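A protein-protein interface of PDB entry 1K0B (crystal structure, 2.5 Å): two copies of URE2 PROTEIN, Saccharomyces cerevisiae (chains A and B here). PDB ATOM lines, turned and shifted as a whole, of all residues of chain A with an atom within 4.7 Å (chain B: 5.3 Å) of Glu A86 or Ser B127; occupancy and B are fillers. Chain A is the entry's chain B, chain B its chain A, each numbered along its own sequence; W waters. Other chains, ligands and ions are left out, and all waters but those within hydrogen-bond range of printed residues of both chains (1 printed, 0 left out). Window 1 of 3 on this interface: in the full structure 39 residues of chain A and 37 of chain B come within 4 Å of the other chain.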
ATOM      1  N   ASN A  68      18.544 -16.327  12.623  1.00  0.00           N
ATOM      2  CA  ASN A  68      17.429 -17.188  12.235  1.00  0.00           C
ATOM      3  C   ASN A  68      16.939 -16.959  10.786  1.00  0.00           C
ATOM      4  O   ASN A  68      16.068 -17.678  10.297  1.00  0.00           O
ATOM      5  CB  ASN A  68      16.272 -16.993  13.216  1.00  0.00           C
ATOM      6  CG  ASN A  68      15.207 -18.069  13.090  1.00  0.00           C
ATOM      7  OD1 ASN A  68      14.048 -17.849  13.448  1.00  0.00           O
ATOM      8  ND2 ASN A  68      15.596 -19.243  12.591  1.00  0.00           N
ATOM      9  N   PRO A  72      10.125 -10.619  11.228  1.00  0.00           N
ATOM     10  CA  PRO A  72      10.805  -9.324  11.155  1.00  0.00           C
ATOM     11  C   PRO A  72      12.167  -9.228  11.832  1.00  0.00           C
ATOM     12  O   PRO A  72      12.564 -10.080  12.631  1.00  0.00           O
ATOM     13  CB  PRO A  72       9.808  -8.389  11.821  1.00  0.00           C
ATOM     14  CG  PRO A  72       9.295  -9.233  12.927  1.00  0.00           C
ATOM     15  CD  PRO A  72       9.026 -10.554  12.209  1.00  0.00           C
ATOM     16  N   ILE A  84      17.768  -6.215  16.308  1.00  0.00           N
ATOM     17  CA  ILE A  84      16.873  -7.057  17.099  1.00  0.00           C
ATOM     18  C   ILE A  84      16.072  -7.926  16.128  1.00  0.00           C
ATOM     19  O   ILE A  84      15.464  -7.404  15.194  1.00  0.00           O
ATOM     20  CB  ILE A  84      15.908  -6.209  17.970  1.00  0.00           C
ATOM     21  CG1 ILE A  84      16.700  -5.215  18.820  1.00  0.00           C
ATOM     22  CG2 ILE A  84      15.121  -7.109  18.910  1.00  0.00           C
ATOM     23  CD1 ILE A  84      17.194  -4.009  18.063  1.00  0.00           C
ATOM     24  N   TRP A  85      16.056  -9.241  16.351  1.00  0.00           N
ATOM     25  CA  TRP A  85      15.368 -10.144  15.423  1.00  0.00           C
ATOM     26  C   TRP A  85      14.103 -10.919  15.804  1.00  0.00           C
ATOM     27  O   TRP A  85      13.700 -11.821  15.074  1.00  0.00           O
ATOM     28  CB  TRP A  85      16.372 -11.137  14.828  1.00  0.00           C
ATOM     29  CG  TRP A  85      17.363 -11.681  15.813  1.00  0.00           C
ATOM     30  CD1 TRP A  85      18.437 -11.025  16.337  1.00  0.00           C
ATOM     31  CD2 TRP A  85      17.366 -12.987  16.396  1.00  0.00           C
ATOM     32  NE1 TRP A  85      19.108 -11.838  17.209  1.00  0.00           N
ATOM     33  CE2 TRP A  85      18.473 -13.050  17.267  1.00  0.00           C
ATOM     34  CE3 TRP A  85      16.538 -14.114  16.266  1.00  0.00           C
ATOM     35  CZ2 TRP A  85      18.781 -14.199  18.013  1.00  0.00           C
ATOM     36  CZ3 TRP A  85      16.845 -15.261  17.007  1.00  0.00           C
ATOM     37  CH2 TRP A  85      17.960 -15.289  17.871  1.00  0.00           C
ATOM     38  N   GLU A  86      13.467 -10.599  16.920  1.00  0.00           N
ATOM     39  CA  GLU A  86      12.233 -11.296  17.264  1.00  0.00           C
ATOM     40  C   GLU A  86      11.155 -10.254  17.513  1.00  0.00           C
ATOM     41  O   GLU A  86      11.373  -9.301  18.273  1.00  0.00           O
ATOM     42  CB  GLU A  86      12.437 -12.173  18.502  1.00  0.00           C
ATOM     43  CG  GLU A  86      13.076 -13.517  18.188  1.00  0.00           C
ATOM     44  CD  GLU A  86      12.080 -14.528  17.629  1.00  0.00           C
ATOM     45  OE1 GLU A  86      12.517 -15.472  16.937  1.00  0.00           O
ATOM     46  OE2 GLU A  86      10.865 -14.390  17.895  1.00  0.00           O
ATOM     47  N   SER A  87      10.000 -10.423  16.872  1.00  0.00           N
ATOM     48  CA  SER A  87       8.916  -9.455  17.035  1.00  0.00           C
ATOM     49  C   SER A  87       8.693  -9.106  18.503  1.00  0.00           C
ATOM     50  O   SER A  87       8.509  -7.935  18.839  1.00  0.00           O
ATOM     51  CB  SER A  87       7.617  -9.976  16.412  1.00  0.00           C
ATOM     52  OG  SER A  87       7.138 -11.118  17.086  1.00  0.00           O
ATOM     53  N   GLY A  88       8.731 -10.116  19.371  1.00  0.00           N
ATOM     54  CA  GLY A  88       8.538  -9.890  20.793  1.00  0.00           C
ATOM     55  C   GLY A  88       9.679  -9.098  21.412  1.00  0.00           C
ATOM     56  O   GLY A  88       9.460  -8.264  22.294  1.00  0.00           O
ATOM     57  N   ALA A  89      10.901  -9.354  20.959  1.00  0.00           N
ATOM     58  CA  ALA A  89      12.066  -8.647  21.488  1.00  0.00           C
ATOM     59  C   ALA A  89      12.141  -7.243  20.900  1.00  0.00           C
ATOM     60  O   ALA A  89      12.690  -6.328  21.515  1.00  0.00           O
ATOM     61  CB  ALA A  89      13.347  -9.420  21.173  1.00  0.00           C
ATOM     62  N   ILE A  90      11.594  -7.073  19.704  1.00  0.00           N
ATOM     63  CA  ILE A  90      11.587  -5.769  19.064  1.00  0.00           C
ATOM     64  C   ILE A  90      10.626  -4.836  19.810  1.00  0.00           C
ATOM     65  O   ILE A  90      10.979  -3.692  20.116  1.00  0.00           O
ATOM     66  CB  ILE A  90      11.191  -5.894  17.564  1.00  0.00           C
ATOM     67  CG1 ILE A  90      12.356  -6.514  16.782  1.00  0.00           C
ATOM     68  CG2 ILE A  90      10.831  -4.532  16.978  1.00  0.00           C
ATOM     69  CD1 ILE A  90      11.985  -6.984  15.395  1.00  0.00           C
ATOM     70  N   THR A 126       3.193 -14.671  21.241  1.00  0.00           N
ATOM     71  CA  THR A 126       4.288 -15.113  20.393  1.00  0.00           C
ATOM     72  C   THR A 126       4.552 -16.607  20.479  1.00  0.00           C
ATOM     73  O   THR A 126       5.041 -17.207  19.526  1.00  0.00           O
ATOM     74  CB  THR A 126       5.593 -14.382  20.756  1.00  0.00           C
ATOM     75  OG1 THR A 126       5.899 -14.608  22.140  1.00  0.00           O
ATOM     76  CG2 THR A 126       5.445 -12.892  20.507  1.00  0.00           C
ATOM     77  N   SER A 127       4.210 -17.202  21.618  1.00  0.00           N
ATOM     78  CA  SER A 127       4.459 -18.618  21.848  1.00  0.00           C
ATOM     79  C   SER A 127       3.276 -19.538  21.658  1.00  0.00           C
ATOM     80  O   SER A 127       3.435 -20.647  21.147  1.00  0.00           O
ATOM     81  CB  SER A 127       5.007 -18.817  23.255  1.00  0.00           C
ATOM     82  OG  SER A 127       6.187 -18.061  23.418  1.00  0.00           O
ATOM     83  N   PRO A 131       2.328 -19.158  16.750  1.00  0.00           N
ATOM     84  CA  PRO A 131       2.750 -20.487  16.294  1.00  0.00           C
ATOM     85  C   PRO A 131       1.608 -21.452  15.945  1.00  0.00           C
ATOM     86  O   PRO A 131       1.665 -22.130  14.919  1.00  0.00           O
ATOM     87  CB  PRO A 131       3.619 -20.995  17.452  1.00  0.00           C
ATOM     88  CG  PRO A 131       4.173 -19.723  18.037  1.00  0.00           C
ATOM     89  CD  PRO A 131       2.961 -18.817  18.036  1.00  0.00           C
ATOM     90  N   ASN B 119      16.709 -10.942  24.983  1.00  0.00           N
ATOM     91  CA  ASN B 119      15.291 -11.120  24.709  1.00  0.00           C
ATOM     92  C   ASN B 119      15.075 -11.774  23.357  1.00  0.00           C
ATOM     93  O   ASN B 119      14.176 -12.595  23.200  1.00  0.00           O
ATOM     94  CB  ASN B 119      14.586  -9.770  24.752  1.00  0.00           C
ATOM     95  CG  ASN B 119      14.367  -9.293  26.152  1.00  0.00           C
ATOM     96  OD1 ASN B 119      14.127  -8.114  26.389  1.00  0.00           O
ATOM     97  ND2 ASN B 119      14.430 -10.219  27.099  1.00  0.00           N
ATOM     98  N   ALA B 120      15.900 -11.399  22.384  1.00  0.00           N
ATOM     99  CA  ALA B 120      15.797 -11.972  21.053  1.00  0.00           C
ATOM    100  C   ALA B 120      15.971 -13.491  21.163  1.00  0.00           C
ATOM    101  O   ALA B 120      15.122 -14.246  20.685  1.00  0.00           O
ATOM    102  CB  ALA B 120      16.856 -11.365  20.129  1.00  0.00           C
ATOM    103  N   LEU B 122      15.698 -15.256  23.818  1.00  0.00           N
ATOM    104  CA  LEU B 122      14.680 -15.797  24.719  1.00  0.00           C
ATOM    105  C   LEU B 122      13.348 -16.001  23.995  1.00  0.00           C
ATOM    106  O   LEU B 122      12.692 -17.027  24.182  1.00  0.00           O
ATOM    107  CB  LEU B 122      14.484 -14.883  25.923  1.00  0.00           C
ATOM    108  CG  LEU B 122      13.542 -15.416  26.997  1.00  0.00           C
ATOM    109  CD1 LEU B 122      14.055 -16.760  27.543  1.00  0.00           C
ATOM    110  CD2 LEU B 122      13.430 -14.371  28.107  1.00  0.00           C
ATOM    111  N   PHE B 123      12.946 -15.031  23.172  1.00  0.00           N
ATOM    112  CA  PHE B 123      11.708 -15.186  22.419  1.00  0.00           C
ATOM    113  C   PHE B 123      11.916 -16.292  21.390  1.00  0.00           C
ATOM    114  O   PHE B 123      11.011 -17.089  21.125  1.00  0.00           O
ATOM    115  CB  PHE B 123      11.320 -13.896  21.703  1.00  0.00           C
ATOM    116  CG  PHE B 123      10.472 -12.981  22.528  1.00  0.00           C
ATOM    117  CD1 PHE B 123      11.050 -11.981  23.302  1.00  0.00           C
ATOM    118  CD2 PHE B 123       9.094 -13.127  22.541  1.00  0.00           C
ATOM    119  CE1 PHE B 123      10.268 -11.139  24.077  1.00  0.00           C
ATOM    120  CE2 PHE B 123       8.303 -12.293  23.311  1.00  0.00           C
ATOM    121  CZ  PHE B 123       8.891 -11.293  24.084  1.00  0.00           C
ATOM    122  N   PHE B 124      13.116 -16.340  20.815  1.00  0.00           N
ATOM    123  CA  PHE B 124      13.437 -17.372  19.840  1.00  0.00           C
ATOM    124  C   PHE B 124      13.228 -18.747  20.473  1.00  0.00           C
ATOM    125  O   PHE B 124      12.661 -19.638  19.864  1.00  0.00           O
ATOM    126  CB  PHE B 124      14.887 -17.234  19.387  1.00  0.00           C
ATOM    127  CG  PHE B 124      15.290 -18.234  18.351  1.00  0.00           C
ATOM    128  CD1 PHE B 124      14.525 -18.409  17.197  1.00  0.00           C
ATOM    129  CD2 PHE B 124      16.436 -19.008  18.516  1.00  0.00           C
ATOM    130  CE1 PHE B 124      14.902 -19.354  16.216  1.00  0.00           C
ATOM    131  CE2 PHE B 124      16.821 -19.955  17.539  1.00  0.00           C
ATOM    132  CZ  PHE B 124      16.052 -20.125  16.393  1.00  0.00           C
ATOM    133  N   GLN B 125      13.673 -18.902  21.716  1.00  0.00           N
ATOM    134  CA  GLN B 125      13.550 -20.168  22.421  1.00  0.00           C
ATOM    135  C   GLN B 125      12.107 -20.525  22.783  1.00  0.00           C
ATOM    136  O   GLN B 125      11.639 -21.624  22.479  1.00  0.00           O
ATOM    137  CB  GLN B 125      14.427 -20.146  23.682  1.00  0.00           C
ATOM    138  CG  GLN B 125      14.664 -21.514  24.312  1.00  0.00           C
ATOM    139  CD  GLN B 125      13.453 -22.036  25.064  1.00  0.00           C
ATOM    140  OE1 GLN B 125      13.085 -23.213  24.945  1.00  0.00           O
ATOM    141  NE2 GLN B 125      12.830 -21.165  25.852  1.00  0.00           N
ATOM    142  N   THR B 126      11.390 -19.608  23.420  1.00  0.00           N
ATOM    143  CA  THR B 126      10.016 -19.898  23.805  1.00  0.00           C
ATOM    144  C   THR B 126       9.047 -19.965  22.627  1.00  0.00           C
ATOM    145  O   THR B 126       8.033 -20.661  22.691  1.00  0.00           O
ATOM    146  CB  THR B 126       9.467 -18.852  24.790  1.00  0.00           C
ATOM    147  OG1 THR B 126       9.290 -17.608  24.104  1.00  0.00           O
ATOM    148  CG2 THR B 126      10.423 -18.654  25.958  1.00  0.00           C
ATOM    149  N   SER B 127       9.355 -19.266  21.544  1.00  0.00           N
ATOM    150  CA  SER B 127       8.440 -19.248  20.408  1.00  0.00           C
ATOM    151  C   SER B 127       8.834 -20.062  19.182  1.00  0.00           C
ATOM    152  O   SER B 127       7.974 -20.435  18.391  1.00  0.00           O
ATOM    153  CB  SER B 127       8.173 -17.796  19.986  1.00  0.00           C
ATOM    154  OG  SER B 127       9.344 -17.167  19.490  1.00  0.00           O
ATOM    155  N   GLY B 128      10.120 -20.338  19.013  1.00  0.00           N
ATOM    156  CA  GLY B 128      10.536 -21.097  17.848  1.00  0.00           C
ATOM    157  C   GLY B 128      11.275 -22.392  18.129  1.00  0.00           C
ATOM    158  O   GLY B 128      11.544 -23.158  17.206  1.00  0.00           O
ATOM    159  N   HIS B 129      11.589 -22.651  19.394  1.00  0.00           N
ATOM    160  CA  HIS B 129      12.326 -23.853  19.772  1.00  0.00           C
ATOM    161  C   HIS B 129      11.481 -24.815  20.610  1.00  0.00           C
ATOM    162  O   HIS B 129      11.409 -26.006  20.305  1.00  0.00           O
ATOM    163  CB  HIS B 129      13.611 -23.431  20.506  1.00  0.00           C
ATOM    164  CG  HIS B 129      14.402 -24.561  21.091  1.00  0.00           C
ATOM    165  ND1 HIS B 129      14.183 -25.043  22.364  1.00  0.00           N
ATOM    166  CD2 HIS B 129      15.463 -25.251  20.606  1.00  0.00           C
ATOM    167  CE1 HIS B 129      15.079 -25.975  22.642  1.00  0.00           C
ATOM    168  NE2 HIS B 129      15.868 -26.120  21.592  1.00  0.00           N
ATOM    169  N   ALA B 130      10.824 -24.302  21.647  1.00  0.00           N
ATOM    170  CA  ALA B 130       9.991 -25.145  22.509  1.00  0.00           C
ATOM    171  C   ALA B 130       8.721 -25.660  21.819  1.00  0.00           C
ATOM    172  O   ALA B 130       8.413 -26.856  21.887  1.00  0.00           O
ATOM    173  CB  ALA B 130       9.624 -24.389  23.777  1.00  0.00           C
ATOM    174  N   PRO B 131       7.963 -24.770  21.151  1.00  0.00           N
ATOM    175  CA  PRO B 131       6.744 -25.241  20.482  1.00  0.00           C
ATOM    176  C   PRO B 131       7.048 -26.334  19.451  1.00  0.00           C
ATOM    177  O   PRO B 131       6.358 -27.357  19.393  1.00  0.00           O
ATOM    178  CB  PRO B 131       6.179 -23.967  19.839  1.00  0.00           C
ATOM    179  CG  PRO B 131       6.694 -22.876  20.726  1.00  0.00           C
ATOM    180  CD  PRO B 131       8.122 -23.313  20.981  1.00  0.00           C
HETATM  181  O   HOH W   1      14.331  -6.358  23.977  1.00  0.00           O
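The side-chain hydroxyl (OG1) of Thr B126 sits at hydrogen-bond distance from the side-chain hydroxyl (OG) of Ser A127 (3.2 Å).
The backbone NH of His B129 sits at hydrogen-bond distance from the backbone carbonyl oxygen of Phe B124, 3.2 Å away. OG1 of Thr B126 sits close to O of Leu B122 (3.5 Å). O of Phe B123 is in hydrogen-bond range of OG1 of Thr B126.
Asn A68 touches Phe B124 (OD1 to CE1, 3.3 Å). Ala B120 touches Trp A85. Glu A86 touches Ala B120 (CG to O, 3.3 Å). Glu A86 touches Phe B124 (OE1 to CD1, 3.6 Å). Ala A89 touches Asn B119 (CB to C, 3.6 Å). Ala B120 touches Ala A89. OG1 of Thr A126 touches CE2 of Phe B123, at 3.5 Å. Ser B127 touches Thr A126 (CB to O, 3.2 Å). Ser B127 touches Ser A127. CG of Pro B131 touches O of Ser A127, 3.97 Å away.
Of the printed residues of chain A, Ser B127 touches Glu A86 (3.5 Å), Thr A126 (3.2 Å), Ser A127 (3.9 Å) and Pro A131 (3.9 Å). Of the printed residues of chain B, Gly A88 touches Phe B123 (3.4 Å). Printed residues of chain B within 4 Å of Trp A85: Ala B120 (3.7 Å) and Phe B124 (3.6 Å). Printed residues of chain A within 4 Å of Ala B120: Trp A85 (3.7 Å), Glu A86 (3.3 Å) and Ala A89 (3.4 Å). Of the printed residues of chain B, Asn A68 touches Phe B124. Gly B128 touches none of the printed residues of chain A. Ala B130 touches none of the printed residues of chain A. The nearest printed residue of chain B that does not touch Ala A89 is Leu B122 (6.8 Å).
Of the 12 printed residues of chain B, 7 touch a printed residue of chain A. Hydrophobic or aromatic side chains of chain B that line the printed part of chain A: Ala B120, Phe B123, Phe B124 and Pro B131. Of the 12 printed residues of chain A, 8 touch a printed residue of chain B. Hydrophobic or aromatic side chains of chain A within 4 Å of the printed part of chain B: Trp A85, Ala A89 and Pro A131. Among the printed residues, 17 pairs touch across the chains.
Thr A126 touches Ser B127, and with the chains exchanged Ser A127 touches Thr B126. Ser B127 touches its own counterpart, Ser A127. Ser A127 touches Pro B131, and with the chains exchanged Pro A131 touches Ser B127. Of the 17 pairs that touch across the chains among the printed residues, 5 have their exchanged pair printed and touching as well.
Water W1 bridges O of Ala A89 (3.0 Å) and OD1 of Asn B119 (3.0 Å).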
